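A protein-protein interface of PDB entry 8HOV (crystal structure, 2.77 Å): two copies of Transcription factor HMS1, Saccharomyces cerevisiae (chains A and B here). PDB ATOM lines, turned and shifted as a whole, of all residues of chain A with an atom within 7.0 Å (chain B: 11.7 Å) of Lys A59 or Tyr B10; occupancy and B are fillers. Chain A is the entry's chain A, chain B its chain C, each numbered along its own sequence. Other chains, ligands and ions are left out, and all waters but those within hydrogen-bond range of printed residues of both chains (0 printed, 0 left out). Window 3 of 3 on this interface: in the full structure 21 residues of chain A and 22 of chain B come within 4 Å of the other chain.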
ATOM      1  N   ARG A  11       7.100 -16.785  16.224  1.00  0.00           N
ATOM      2  CA  ARG A  11       7.225 -18.071  16.902  1.00  0.00           C
ATOM      3  C   ARG A  11       8.524 -18.775  16.528  1.00  0.00           C
ATOM      4  O   ARG A  11       9.157 -19.411  17.379  1.00  0.00           O
ATOM      5  CB  ARG A  11       6.018 -18.952  16.580  1.00  0.00           C
ATOM      6  CG  ARG A  11       4.739 -18.523  17.287  1.00  0.00           C
ATOM      7  CD  ARG A  11       3.567 -19.435  16.948  1.00  0.00           C
ATOM      8  NE  ARG A  11       3.051 -19.202  15.604  1.00  0.00           N
ATOM      9  CZ  ARG A  11       3.373 -19.924  14.540  1.00  0.00           C
ATOM     10  NH1 ARG A  11       4.218 -20.939  14.622  1.00  0.00           N
ATOM     11  NH2 ARG A  11       2.832 -19.622  13.363  1.00  0.00           N
ATOM     12  N   ILE A  14      11.677 -17.332  18.445  1.00  0.00           N
ATOM     13  CA  ILE A  14      11.814 -17.832  19.812  1.00  0.00           C
ATOM     14  C   ILE A  14      12.367 -19.252  19.807  1.00  0.00           C
ATOM     15  O   ILE A  14      13.276 -19.587  20.575  1.00  0.00           O
ATOM     16  CB  ILE A  14      10.464 -17.761  20.548  1.00  0.00           C
ATOM     17  CG1 ILE A  14       9.997 -16.310  20.679  1.00  0.00           C
ATOM     18  CG2 ILE A  14      10.567 -18.420  21.916  1.00  0.00           C
ATOM     19  CD1 ILE A  14       8.666 -16.161  21.386  1.00  0.00           C
ATOM     20  N   ASN A  15      11.824 -20.109  18.936  1.00  0.00           N
ATOM     21  CA  ASN A  15      12.241 -21.508  18.911  1.00  0.00           C
ATOM     22  C   ASN A  15      13.678 -21.666  18.433  1.00  0.00           C
ATOM     23  O   ASN A  15      14.355 -22.621  18.827  1.00  0.00           O
ATOM     24  CB  ASN A  15      11.298 -22.322  18.027  1.00  0.00           C
ATOM     25  CG  ASN A  15       9.883 -22.359  18.567  1.00  0.00           C
ATOM     26  OD1 ASN A  15       9.669 -22.305  19.779  1.00  0.00           O
ATOM     27  ND2 ASN A  15       8.908 -22.449  17.669  1.00  0.00           N
ATOM     28  N   ILE A  18      15.685 -21.233  21.614  1.00  0.00           N
ATOM     29  CA  ILE A  18      15.547 -22.372  22.514  1.00  0.00           C
ATOM     30  C   ILE A  18      16.370 -23.552  22.009  1.00  0.00           C
ATOM     31  O   ILE A  18      17.010 -24.260  22.795  1.00  0.00           O
ATOM     32  CB  ILE A  18      14.062 -22.742  22.688  1.00  0.00           C
ATOM     33  CG1 ILE A  18      13.295 -21.586  23.332  1.00  0.00           C
ATOM     34  CG2 ILE A  18      13.920 -24.002  23.525  1.00  0.00           C
ATOM     35  CD1 ILE A  18      11.848 -21.911  23.642  1.00  0.00           C
ATOM     36  N   LEU A  57      13.459 -33.573  26.689  1.00  0.00           N
ATOM     37  CA  LEU A  57      14.083 -32.516  25.904  1.00  0.00           C
ATOM     38  C   LEU A  57      13.058 -31.506  25.391  1.00  0.00           C
ATOM     39  O   LEU A  57      13.252 -30.895  24.338  1.00  0.00           O
ATOM     40  CB  LEU A  57      14.883 -33.114  24.747  1.00  0.00           C
ATOM     41  CG  LEU A  57      16.245 -32.475  24.468  1.00  0.00           C
ATOM     42  CD1 LEU A  57      17.067 -32.390  25.745  1.00  0.00           C
ATOM     43  CD2 LEU A  57      16.997 -33.256  23.402  1.00  0.00           C
ATOM     44  N   ASN A  58      11.966 -31.317  26.129  1.00  0.00           N
ATOM     45  CA  ASN A  58      10.968 -30.331  25.747  1.00  0.00           C
ATOM     46  C   ASN A  58      11.480 -28.916  26.029  1.00  0.00           C
ATOM     47  O   ASN A  58      12.571 -28.713  26.571  1.00  0.00           O
ATOM     48  CB  ASN A  58       9.653 -30.587  26.484  1.00  0.00           C
ATOM     49  CG  ASN A  58       9.845 -30.756  27.978  1.00  0.00           C
ATOM     50  OD1 ASN A  58      10.021 -29.780  28.706  1.00  0.00           O
ATOM     51  ND2 ASN A  58       9.807 -32.000  28.443  1.00  0.00           N
ATOM     52  N   LYS A  59      10.670 -27.924  25.642  1.00  0.00           N
ATOM     53  CA  LYS A  59      11.064 -26.529  25.819  1.00  0.00           C
ATOM     54  C   LYS A  59      11.278 -26.192  27.289  1.00  0.00           C
ATOM     55  O   LYS A  59      12.259 -25.529  27.645  1.00  0.00           O
ATOM     56  CB  LYS A  59      10.009 -25.598  25.221  1.00  0.00           C
ATOM     57  CG  LYS A  59       9.781 -25.750  23.727  1.00  0.00           C
ATOM     58  CD  LYS A  59       8.672 -24.814  23.265  1.00  0.00           C
ATOM     59  CE  LYS A  59       8.264 -25.081  21.827  1.00  0.00           C
ATOM     60  NZ  LYS A  59       7.068 -24.278  21.446  1.00  0.00           N
ATOM     61  N   ALA A  60      10.364 -26.633  28.158  1.00  0.00           N
ATOM     62  CA  ALA A  60      10.503 -26.349  29.581  1.00  0.00           C
ATOM     63  C   ALA A  60      11.761 -26.991  30.150  1.00  0.00           C
ATOM     64  O   ALA A  60      12.438 -26.401  31.000  1.00  0.00           O
ATOM     65  CB  ALA A  60       9.265 -26.827  30.338  1.00  0.00           C
ATOM     66  N   SER A  61      12.085 -28.206  29.701  1.00  0.00           N
ATOM     67  CA  SER A  61      13.309 -28.861  30.155  1.00  0.00           C
ATOM     68  C   SER A  61      14.546 -28.089  29.715  1.00  0.00           C
ATOM     69  O   SER A  61      15.517 -27.977  30.471  1.00  0.00           O
ATOM     70  CB  SER A  61      13.362 -30.297  29.635  1.00  0.00           C
ATOM     71  OG  SER A  61      12.358 -31.094  30.238  1.00  0.00           O
ATOM     72  N   ILE A  62      14.537 -27.563  28.488  1.00  0.00           N
ATOM     73  CA  ILE A  62      15.676 -26.785  28.008  1.00  0.00           C
ATOM     74  C   ILE A  62      15.872 -25.545  28.871  1.00  0.00           C
ATOM     75  O   ILE A  62      17.004 -25.174  29.204  1.00  0.00           O
ATOM     76  CB  ILE A  62      15.486 -26.428  26.521  1.00  0.00           C
ATOM     77  CG1 ILE A  62      15.459 -27.701  25.672  1.00  0.00           C
ATOM     78  CG2 ILE A  62      16.584 -25.485  26.042  1.00  0.00           C
ATOM     79  CD1 ILE A  62      15.310 -27.447  24.189  1.00  0.00           C
ATOM     80  N   LEU A  63      14.775 -24.891  29.254  1.00  0.00           N
ATOM     81  CA  LEU A  63      14.875 -23.683  30.065  1.00  0.00           C
ATOM     82  C   LEU A  63      15.384 -23.992  31.468  1.00  0.00           C
ATOM     83  O   LEU A  63      16.294 -23.322  31.968  1.00  0.00           O
ATOM     84  CB  LEU A  63      13.519 -22.979  30.124  1.00  0.00           C
ATOM     85  CG  LEU A  63      12.940 -22.494  28.791  1.00  0.00           C
ATOM     86  CD1 LEU A  63      11.619 -21.775  29.006  1.00  0.00           C
ATOM     87  CD2 LEU A  63      13.930 -21.598  28.064  1.00  0.00           C
ATOM     88  N   THR A  64      14.810 -25.008  32.122  1.00  0.00           N
ATOM     89  CA  THR A  64      15.176 -25.282  33.509  1.00  0.00           C
ATOM     90  C   THR A  64      16.609 -25.786  33.631  1.00  0.00           C
ATOM     91  O   THR A  64      17.278 -25.504  34.632  1.00  0.00           O
ATOM     92  CB  THR A  64      14.198 -26.282  34.136  1.00  0.00           C
ATOM     93  OG1 THR A  64      14.536 -26.478  35.515  1.00  0.00           O
ATOM     94  CG2 THR A  64      14.242 -27.618  33.419  1.00  0.00           C
ATOM     95  N   ASN B   4      -9.136 -25.263  27.997  1.00  0.00           N
ATOM     96  CA  ASN B   4      -8.378 -26.315  28.725  1.00  0.00           C
ATOM     97  C   ASN B   4      -7.512 -25.668  29.809  1.00  0.00           C
ATOM     98  O   ASN B   4      -6.614 -24.885  29.451  1.00  0.00           O
ATOM     99  CB  ASN B   4      -7.516 -27.164  27.786  1.00  0.00           C
ATOM    100  CG  ASN B   4      -8.311 -28.189  27.007  1.00  0.00           C
ATOM    101  OD1 ASN B   4      -9.486 -28.415  27.285  1.00  0.00           O
ATOM    102  ND2 ASN B   4      -7.675 -28.820  26.034  1.00  0.00           N
ATOM    103  N   ILE B   5      -7.776 -25.985  31.078  1.00  0.00           N
ATOM    104  CA  ILE B   5      -6.920 -25.465  32.181  1.00  0.00           C
ATOM    105  C   ILE B   5      -5.530 -26.082  32.028  1.00  0.00           C
ATOM    106  O   ILE B   5      -4.538 -25.354  32.178  1.00  0.00           O
ATOM    107  CB  ILE B   5      -7.536 -25.796  33.551  1.00  0.00           C
ATOM    108  CG1 ILE B   5      -8.917 -25.156  33.713  1.00  0.00           C
ATOM    109  CG2 ILE B   5      -6.597 -25.396  34.677  1.00  0.00           C
ATOM    110  CD1 ILE B   5      -8.919 -23.657  33.531  1.00  0.00           C
ATOM    111  N   ILE B   6      -5.474 -27.378  31.732  1.00  0.00           N
ATOM    112  CA  ILE B   6      -4.165 -28.053  31.518  1.00  0.00           C
ATOM    113  C   ILE B   6      -3.323 -27.164  30.612  1.00  0.00           C
ATOM    114  O   ILE B   6      -2.185 -26.850  30.989  1.00  0.00           O
ATOM    115  CB  ILE B   6      -4.359 -29.447  30.897  1.00  0.00           C
ATOM    116  CG1 ILE B   6      -5.068 -30.403  31.860  1.00  0.00           C
ATOM    117  CG2 ILE B   6      -3.029 -30.012  30.427  1.00  0.00           C
ATOM    118  CD1 ILE B   6      -4.257 -30.741  33.088  1.00  0.00           C
ATOM    119  N   GLU B   7      -3.867 -26.770  29.464  1.00  0.00           N
ATOM    120  CA  GLU B   7      -3.028 -26.006  28.548  1.00  0.00           C
ATOM    121  C   GLU B   7      -2.474 -24.741  29.196  1.00  0.00           C
ATOM    122  O   GLU B   7      -1.377 -24.297  28.838  1.00  0.00           O
ATOM    123  CB  GLU B   7      -3.816 -25.661  27.285  1.00  0.00           C
ATOM    124  CG  GLU B   7      -4.171 -26.869  26.433  1.00  0.00           C
ATOM    125  CD  GLU B   7      -5.013 -26.508  25.226  1.00  0.00           C
ATOM    126  OE1 GLU B   7      -5.484 -25.352  25.146  1.00  0.00           O
ATOM    127  OE2 GLU B   7      -5.216 -27.385  24.361  1.00  0.00           O
ATOM    128  N   LYS B   8      -3.208 -24.148  30.142  1.00  0.00           N
ATOM    129  CA  LYS B   8      -2.711 -22.948  30.810  1.00  0.00           C
ATOM    130  C   LYS B   8      -1.478 -23.255  31.651  1.00  0.00           C
ATOM    131  O   LYS B   8      -0.572 -22.419  31.761  1.00  0.00           O
ATOM    132  CB  LYS B   8      -3.806 -22.328  31.678  1.00  0.00           C
ATOM    133  CG  LYS B   8      -3.574 -20.854  31.981  1.00  0.00           C
ATOM    134  CD  LYS B   8      -4.196 -20.438  33.302  1.00  0.00           C
ATOM    135  CE  LYS B   8      -3.426 -21.021  34.477  1.00  0.00           C
ATOM    136  NZ  LYS B   8      -3.925 -20.505  35.781  1.00  0.00           N
ATOM    137  N   LYS B   9      -1.429 -24.444  32.258  1.00  0.00           N
ATOM    138  CA  LYS B   9      -0.267 -24.826  33.052  1.00  0.00           C
ATOM    139  C   LYS B   9       0.987 -24.898  32.191  1.00  0.00           C
ATOM    140  O   LYS B   9       2.074 -24.503  32.628  1.00  0.00           O
ATOM    141  CB  LYS B   9      -0.521 -26.170  33.738  1.00  0.00           C
ATOM    142  CG  LYS B   9      -1.925 -26.330  34.294  1.00  0.00           C
ATOM    143  CD  LYS B   9      -2.140 -27.729  34.848  1.00  0.00           C
ATOM    144  CE  LYS B   9      -3.599 -27.967  35.196  1.00  0.00           C
ATOM    145  NZ  LYS B   9      -4.109 -26.970  36.176  1.00  0.00           N
ATOM    146  N   TYR B  10       0.856 -25.414  30.966  1.00  0.00           N
ATOM    147  CA  TYR B  10       2.003 -25.501  30.068  1.00  0.00           C
ATOM    148  C   TYR B  10       2.545 -24.118  29.725  1.00  0.00           C
ATOM    149  O   TYR B  10       3.763 -23.902  29.735  1.00  0.00           O
ATOM    150  CB  TYR B  10       1.612 -26.260  28.801  1.00  0.00           C
ATOM    151  CG  TYR B  10       2.672 -26.244  27.725  1.00  0.00           C
ATOM    152  CD1 TYR B  10       3.763 -27.100  27.786  1.00  0.00           C
ATOM    153  CD2 TYR B  10       2.577 -25.376  26.645  1.00  0.00           C
ATOM    154  CE1 TYR B  10       4.732 -27.089  26.802  1.00  0.00           C
ATOM    155  CE2 TYR B  10       3.540 -25.359  25.657  1.00  0.00           C
ATOM    156  CZ  TYR B  10       4.614 -26.218  25.739  1.00  0.00           C
ATOM    157  OH  TYR B  10       5.574 -26.199  24.755  1.00  0.00           O
ATOM    158  N   ARG B  11       1.658 -23.171  29.410  1.00  0.00           N
ATOM    159  CA  ARG B  11       2.104 -21.810  29.132  1.00  0.00           C
ATOM    160  C   ARG B  11       2.670 -21.149  30.382  1.00  0.00           C
ATOM    161  O   ARG B  11       3.688 -20.451  30.316  1.00  0.00           O
ATOM    162  CB  ARG B  11       0.951 -20.980  28.568  1.00  0.00           C
ATOM    163  CG  ARG B  11       0.205 -21.644  27.429  1.00  0.00           C
ATOM    164  CD  ARG B  11      -0.858 -20.720  26.858  1.00  0.00           C
ATOM    165  NE  ARG B  11      -1.915 -21.471  26.192  1.00  0.00           N
ATOM    166  CZ  ARG B  11      -3.077 -21.778  26.751  1.00  0.00           C
ATOM    167  NH1 ARG B  11      -3.385 -21.374  27.972  1.00  0.00           N
ATOM    168  NH2 ARG B  11      -3.953 -22.508  26.067  1.00  0.00           N
ATOM    169  N   SER B  12       2.018 -21.353  31.529  1.00  0.00           N
ATOM    170  CA  SER B  12       2.477 -20.733  32.767  1.00  0.00           C
ATOM    171  C   SER B  12       3.857 -21.241  33.166  1.00  0.00           C
ATOM    172  O   SER B  12       4.728 -20.452  33.552  1.00  0.00           O
ATOM    173  CB  SER B  12       1.468 -20.987  33.887  1.00  0.00           C
ATOM    174  OG  SER B  12       1.941 -20.481  35.124  1.00  0.00           O
ATOM    175  N   ASN B  13       4.078 -22.555  33.075  1.00  0.00           N
ATOM    176  CA  ASN B  13       5.358 -23.118  33.492  1.00  0.00           C
ATOM    177  C   ASN B  13       6.496 -22.653  32.593  1.00  0.00           C
ATOM    178  O   ASN B  13       7.622 -22.469  33.068  1.00  0.00           O
ATOM    179  CB  ASN B  13       5.277 -24.644  33.518  1.00  0.00           C
ATOM    180  CG  ASN B  13       6.531 -25.287  34.079  1.00  0.00           C
ATOM    181  OD1 ASN B  13       7.250 -25.993  33.372  1.00  0.00           O
ATOM    182  ND2 ASN B  13       6.802 -25.042  35.357  1.00  0.00           N
ATOM    183  N   ILE B  14       6.228 -22.460  31.300  1.00  0.00           N
ATOM    184  CA  ILE B  14       7.243 -21.890  30.420  1.00  0.00           C
ATOM    185  C   ILE B  14       7.474 -20.422  30.758  1.00  0.00           C
ATOM    186  O   ILE B  14       8.621 -19.964  30.840  1.00  0.00           O
ATOM    187  CB  ILE B  14       6.846 -22.079  28.945  1.00  0.00           C
ATOM    188  CG1 ILE B  14       6.935 -23.556  28.554  1.00  0.00           C
ATOM    189  CG2 ILE B  14       7.729 -21.235  28.040  1.00  0.00           C
ATOM    190  CD1 ILE B  14       6.712 -23.812  27.080  1.00  0.00           C
ATOM    191  N   ASN B  15       6.395 -19.665  30.971  1.00  0.00           N
ATOM    192  CA  ASN B  15       6.539 -18.253  31.310  1.00  0.00           C
ATOM    193  C   ASN B  15       7.247 -18.071  32.645  1.00  0.00           C
ATOM    194  O   ASN B  15       8.050 -17.145  32.807  1.00  0.00           O
ATOM    195  CB  ASN B  15       5.170 -17.572  31.332  1.00  0.00           C
ATOM    196  CG  ASN B  15       4.618 -17.329  29.942  1.00  0.00           C
ATOM    197  OD1 ASN B  15       5.367 -17.269  28.966  1.00  0.00           O
ATOM    198  ND2 ASN B  15       3.301 -17.180  29.845  1.00  0.00           N
ATOM    199  N   ASP B  16       6.965 -18.945  33.615  1.00  0.00           N
ATOM    200  CA  ASP B  16       7.610 -18.833  34.920  1.00  0.00           C
ATOM    201  C   ASP B  16       9.120 -19.002  34.805  1.00  0.00           C
ATOM    202  O   ASP B  16       9.884 -18.301  35.478  1.00  0.00           O
ATOM    203  CB  ASP B  16       7.025 -19.862  35.889  1.00  0.00           C
ATOM    204  CG  ASP B  16       5.607 -19.527  36.310  1.00  0.00           C
ATOM    205  OD1 ASP B  16       5.175 -18.376  36.089  1.00  0.00           O
ATOM    206  OD2 ASP B  16       4.920 -20.416  36.856  1.00  0.00           O
ATOM    207  N   LYS B  17       9.571 -19.929  33.957  1.00  0.00           N
ATOM    208  CA  LYS B  17      11.004 -20.097  33.749  1.00  0.00           C
ATOM    209  C   LYS B  17      11.589 -18.945  32.942  1.00  0.00           C
ATOM    210  O   LYS B  17      12.778 -18.635  33.078  1.00  0.00           O
ATOM    211  CB  LYS B  17      11.280 -21.434  33.064  1.00  0.00           C
ATOM    212  CG  LYS B  17      10.799 -22.635  33.866  1.00  0.00           C
ATOM    213  CD  LYS B  17      11.120 -23.948  33.171  1.00  0.00           C
ATOM    214  CE  LYS B  17      10.627 -25.130  33.988  1.00  0.00           C
ATOM    215  NZ  LYS B  17      11.168 -25.100  35.375  1.00  0.00           N
ATOM    216  N   ILE B  18      10.778 -18.305  32.096  1.00  0.00           N
ATOM    217  CA  ILE B  18      11.230 -17.108  31.393  1.00  0.00           C
ATOM    218  C   ILE B  18      11.496 -15.981  32.384  1.00  0.00           C
ATOM    219  O   ILE B  18      12.500 -15.265  32.281  1.00  0.00           O
ATOM    220  CB  ILE B  18      10.202 -16.693  30.322  1.00  0.00           C
ATOM    221  CG1 ILE B  18      10.163 -17.722  29.189  1.00  0.00           C
ATOM    222  CG2 ILE B  18      10.517 -15.310  29.777  1.00  0.00           C
ATOM    223  CD1 ILE B  18      11.474 -17.867  28.449  1.00  0.00           C
ATOM    224  N   GLU B  19      10.602 -15.808  33.362  1.00  0.00           N
ATOM    225  CA  GLU B  19      10.789 -14.762  34.363  1.00  0.00           C
ATOM    226  C   GLU B  19      12.005 -15.031  35.240  1.00  0.00           C
ATOM    227  O   GLU B  19      12.668 -14.085  35.681  1.00  0.00           O
ATOM    228  CB  GLU B  19       9.533 -14.627  35.225  1.00  0.00           C
ATOM    229  CG  GLU B  19       8.254 -14.447  34.424  1.00  0.00           C
ATOM    230  CD  GLU B  19       8.364 -13.350  33.383  1.00  0.00           C
ATOM    231  OE1 GLU B  19       8.810 -12.237  33.733  1.00  0.00           O
ATOM    232  OE2 GLU B  19       8.015 -13.604  32.211  1.00  0.00           O
ATOM    233  N   GLN B  20      12.307 -16.303  35.510  1.00  0.00           N
ATOM    234  CA  GLN B  20      13.495 -16.629  36.294  1.00  0.00           C
ATOM    235  C   GLN B  20      14.764 -16.192  35.574  1.00  0.00           C
ATOM    236  O   GLN B  20      15.699 -15.686  36.205  1.00  0.00           O
ATOM    237  CB  GLN B  20      13.532 -18.127  36.594  1.00  0.00           C
ATOM    238  CG  GLN B  20      12.399 -18.610  37.482  1.00  0.00           C
ATOM    239  CD  GLN B  20      12.408 -20.116  37.674  1.00  0.00           C
ATOM    240  OE1 GLN B  20      13.436 -20.769  37.495  1.00  0.00           O
ATOM    241  NE2 GLN B  20      11.257 -20.674  38.034  1.00  0.00           N
ATOM    242  N   LEU B  21      14.816 -16.383  34.253  1.00  0.00           N
ATOM    243  CA  LEU B  21      15.961 -15.907  33.482  1.00  0.00           C
ATOM    244  C   LEU B  21      16.085 -14.390  33.563  1.00  0.00           C
ATOM    245  O   LEU B  21      17.196 -13.853  33.629  1.00  0.00           O
ATOM    246  CB  LEU B  21      15.840 -16.358  32.027  1.00  0.00           C
ATOM    247  CG  LEU B  21      16.023 -17.848  31.739  1.00  0.00           C
ATOM    248  CD1 LEU B  21      15.555 -18.180  30.332  1.00  0.00           C
ATOM    249  CD2 LEU B  21      17.478 -18.244  31.923  1.00  0.00           C
ATOM    250  N   LYS B  59      10.316 -11.931  25.225  1.00  0.00           N
ATOM    251  CA  LYS B  59      10.811 -13.297  25.380  1.00  0.00           C
ATOM    252  C   LYS B  59      12.087 -13.521  24.579  1.00  0.00           C
ATOM    253  O   LYS B  59      13.028 -14.162  25.062  1.00  0.00           O
ATOM    254  CB  LYS B  59       9.739 -14.303  24.959  1.00  0.00           C
ATOM    255  CG  LYS B  59       8.581 -14.440  25.931  1.00  0.00           C
ATOM    256  CD  LYS B  59       7.579 -15.464  25.424  1.00  0.00           C
ATOM    257  CE  LYS B  59       6.362 -15.556  26.327  1.00  0.00           C
ATOM    258  NZ  LYS B  59       5.323 -16.456  25.751  1.00  0.00           N
ATOM    259  N   LEU B  63      15.762 -14.634  26.099  1.00  0.00           N
ATOM    260  CA  LEU B  63      16.506 -15.802  25.638  1.00  0.00           C
ATOM    261  C   LEU B  63      17.847 -15.402  25.032  1.00  0.00           C
ATOM    262  O   LEU B  63      18.869 -16.047  25.294  1.00  0.00           O
ATOM    263  CB  LEU B  63      15.674 -16.588  24.625  1.00  0.00           C
ATOM    264  CG  LEU B  63      14.367 -17.192  25.143  1.00  0.00           C
ATOM    265  CD1 LEU B  63      13.566 -17.801  24.003  1.00  0.00           C
ATOM    266  CD2 LEU B  63      14.644 -18.229  26.215  1.00  0.00           C
ATOM    267  N   SER B  66      20.176 -14.476  27.758  1.00  0.00           N
ATOM    268  CA  SER B  66      20.568 -15.675  28.494  1.00  0.00           C
ATOM    269  C   SER B  66      21.655 -16.443  27.754  1.00  0.00           C
ATOM    270  O   SER B  66      22.601 -16.945  28.373  1.00  0.00           O
ATOM    271  CB  SER B  66      19.351 -16.566  28.739  1.00  0.00           C
ATOM    272  OG  SER B  66      18.410 -15.921  29.582  1.00  0.00           O
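N of Ala A60 sits at hydrogen-bond distance from OD1 of Asn A58.
Among the printed residues, merely in contact across the chains: Ile A14 with Leu B63, Ile A18 with Leu B63, Lys A59 with Tyr B10, Ala A60 with Asn B13, Ala A60 with Lys B17, Leu A63 with Ile B14, Leu A63 with Lys B17, Leu A63 with Ile B18, Leu A63 with Leu B63 and Thr A64 with Lys B17.
No residue of chain B comes within 4 Å of Asn A15. Printed residues of chain B within 4 Å of Lys A59: Tyr B10. No residue of chain B comes within 4 Å of Ser A61. No residue of chain B comes within 4 Å of Ile A62. Of the printed residues of chain B, Thr A64 touches Lys B17 (3.5 Å). Of the printed residues of chain A, Lys B17 touches Ala A60 (3.5 Å), Leu A63 (3.997 Å) and Thr A64 (3.5 Å). Printed residues of chain A within 4 Å of Ile B18: Leu A63. Of the printed residues of chain A, Leu B63 touches Ile A14 (3.7 Å), Ile A18 (3.9 Å) and Leu A63 (3.9 Å). The nearest residue of chain A that does not touch Tyr B10 is Ala A60 (5.8 Å). The nearest printed residue of chain A that does not touch Asn B13 is Leu A63 (5.7 Å).
Hydrophobic or aromatic side chains of chain B that line the printed part of chain A: Tyr B10, Ile B18 and Leu B63. Printed residues of chain A that touch a printed residue of chain B: Ile A14, Ile A18, Lys A59, Ala A60, Leu A63 and Thr A64. Hydrophobic or aromatic side chains of chain A within 4 Å of the printed part of chain B: Ile A14, Ile A18, Ala A60 and Leu A63.
Ile A14 touches Leu B63, and with the chains exchanged Leu A63 touches Ile B14. Ile A18 touches Leu B63, and with the chains exchanged Leu A63 touches Ile B18. Leu A63 touches its own counterpart, Leu B63. Of the 10 pairs that touch across the chains among the printed residues, 5 have their exchanged pair printed and touching as well.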
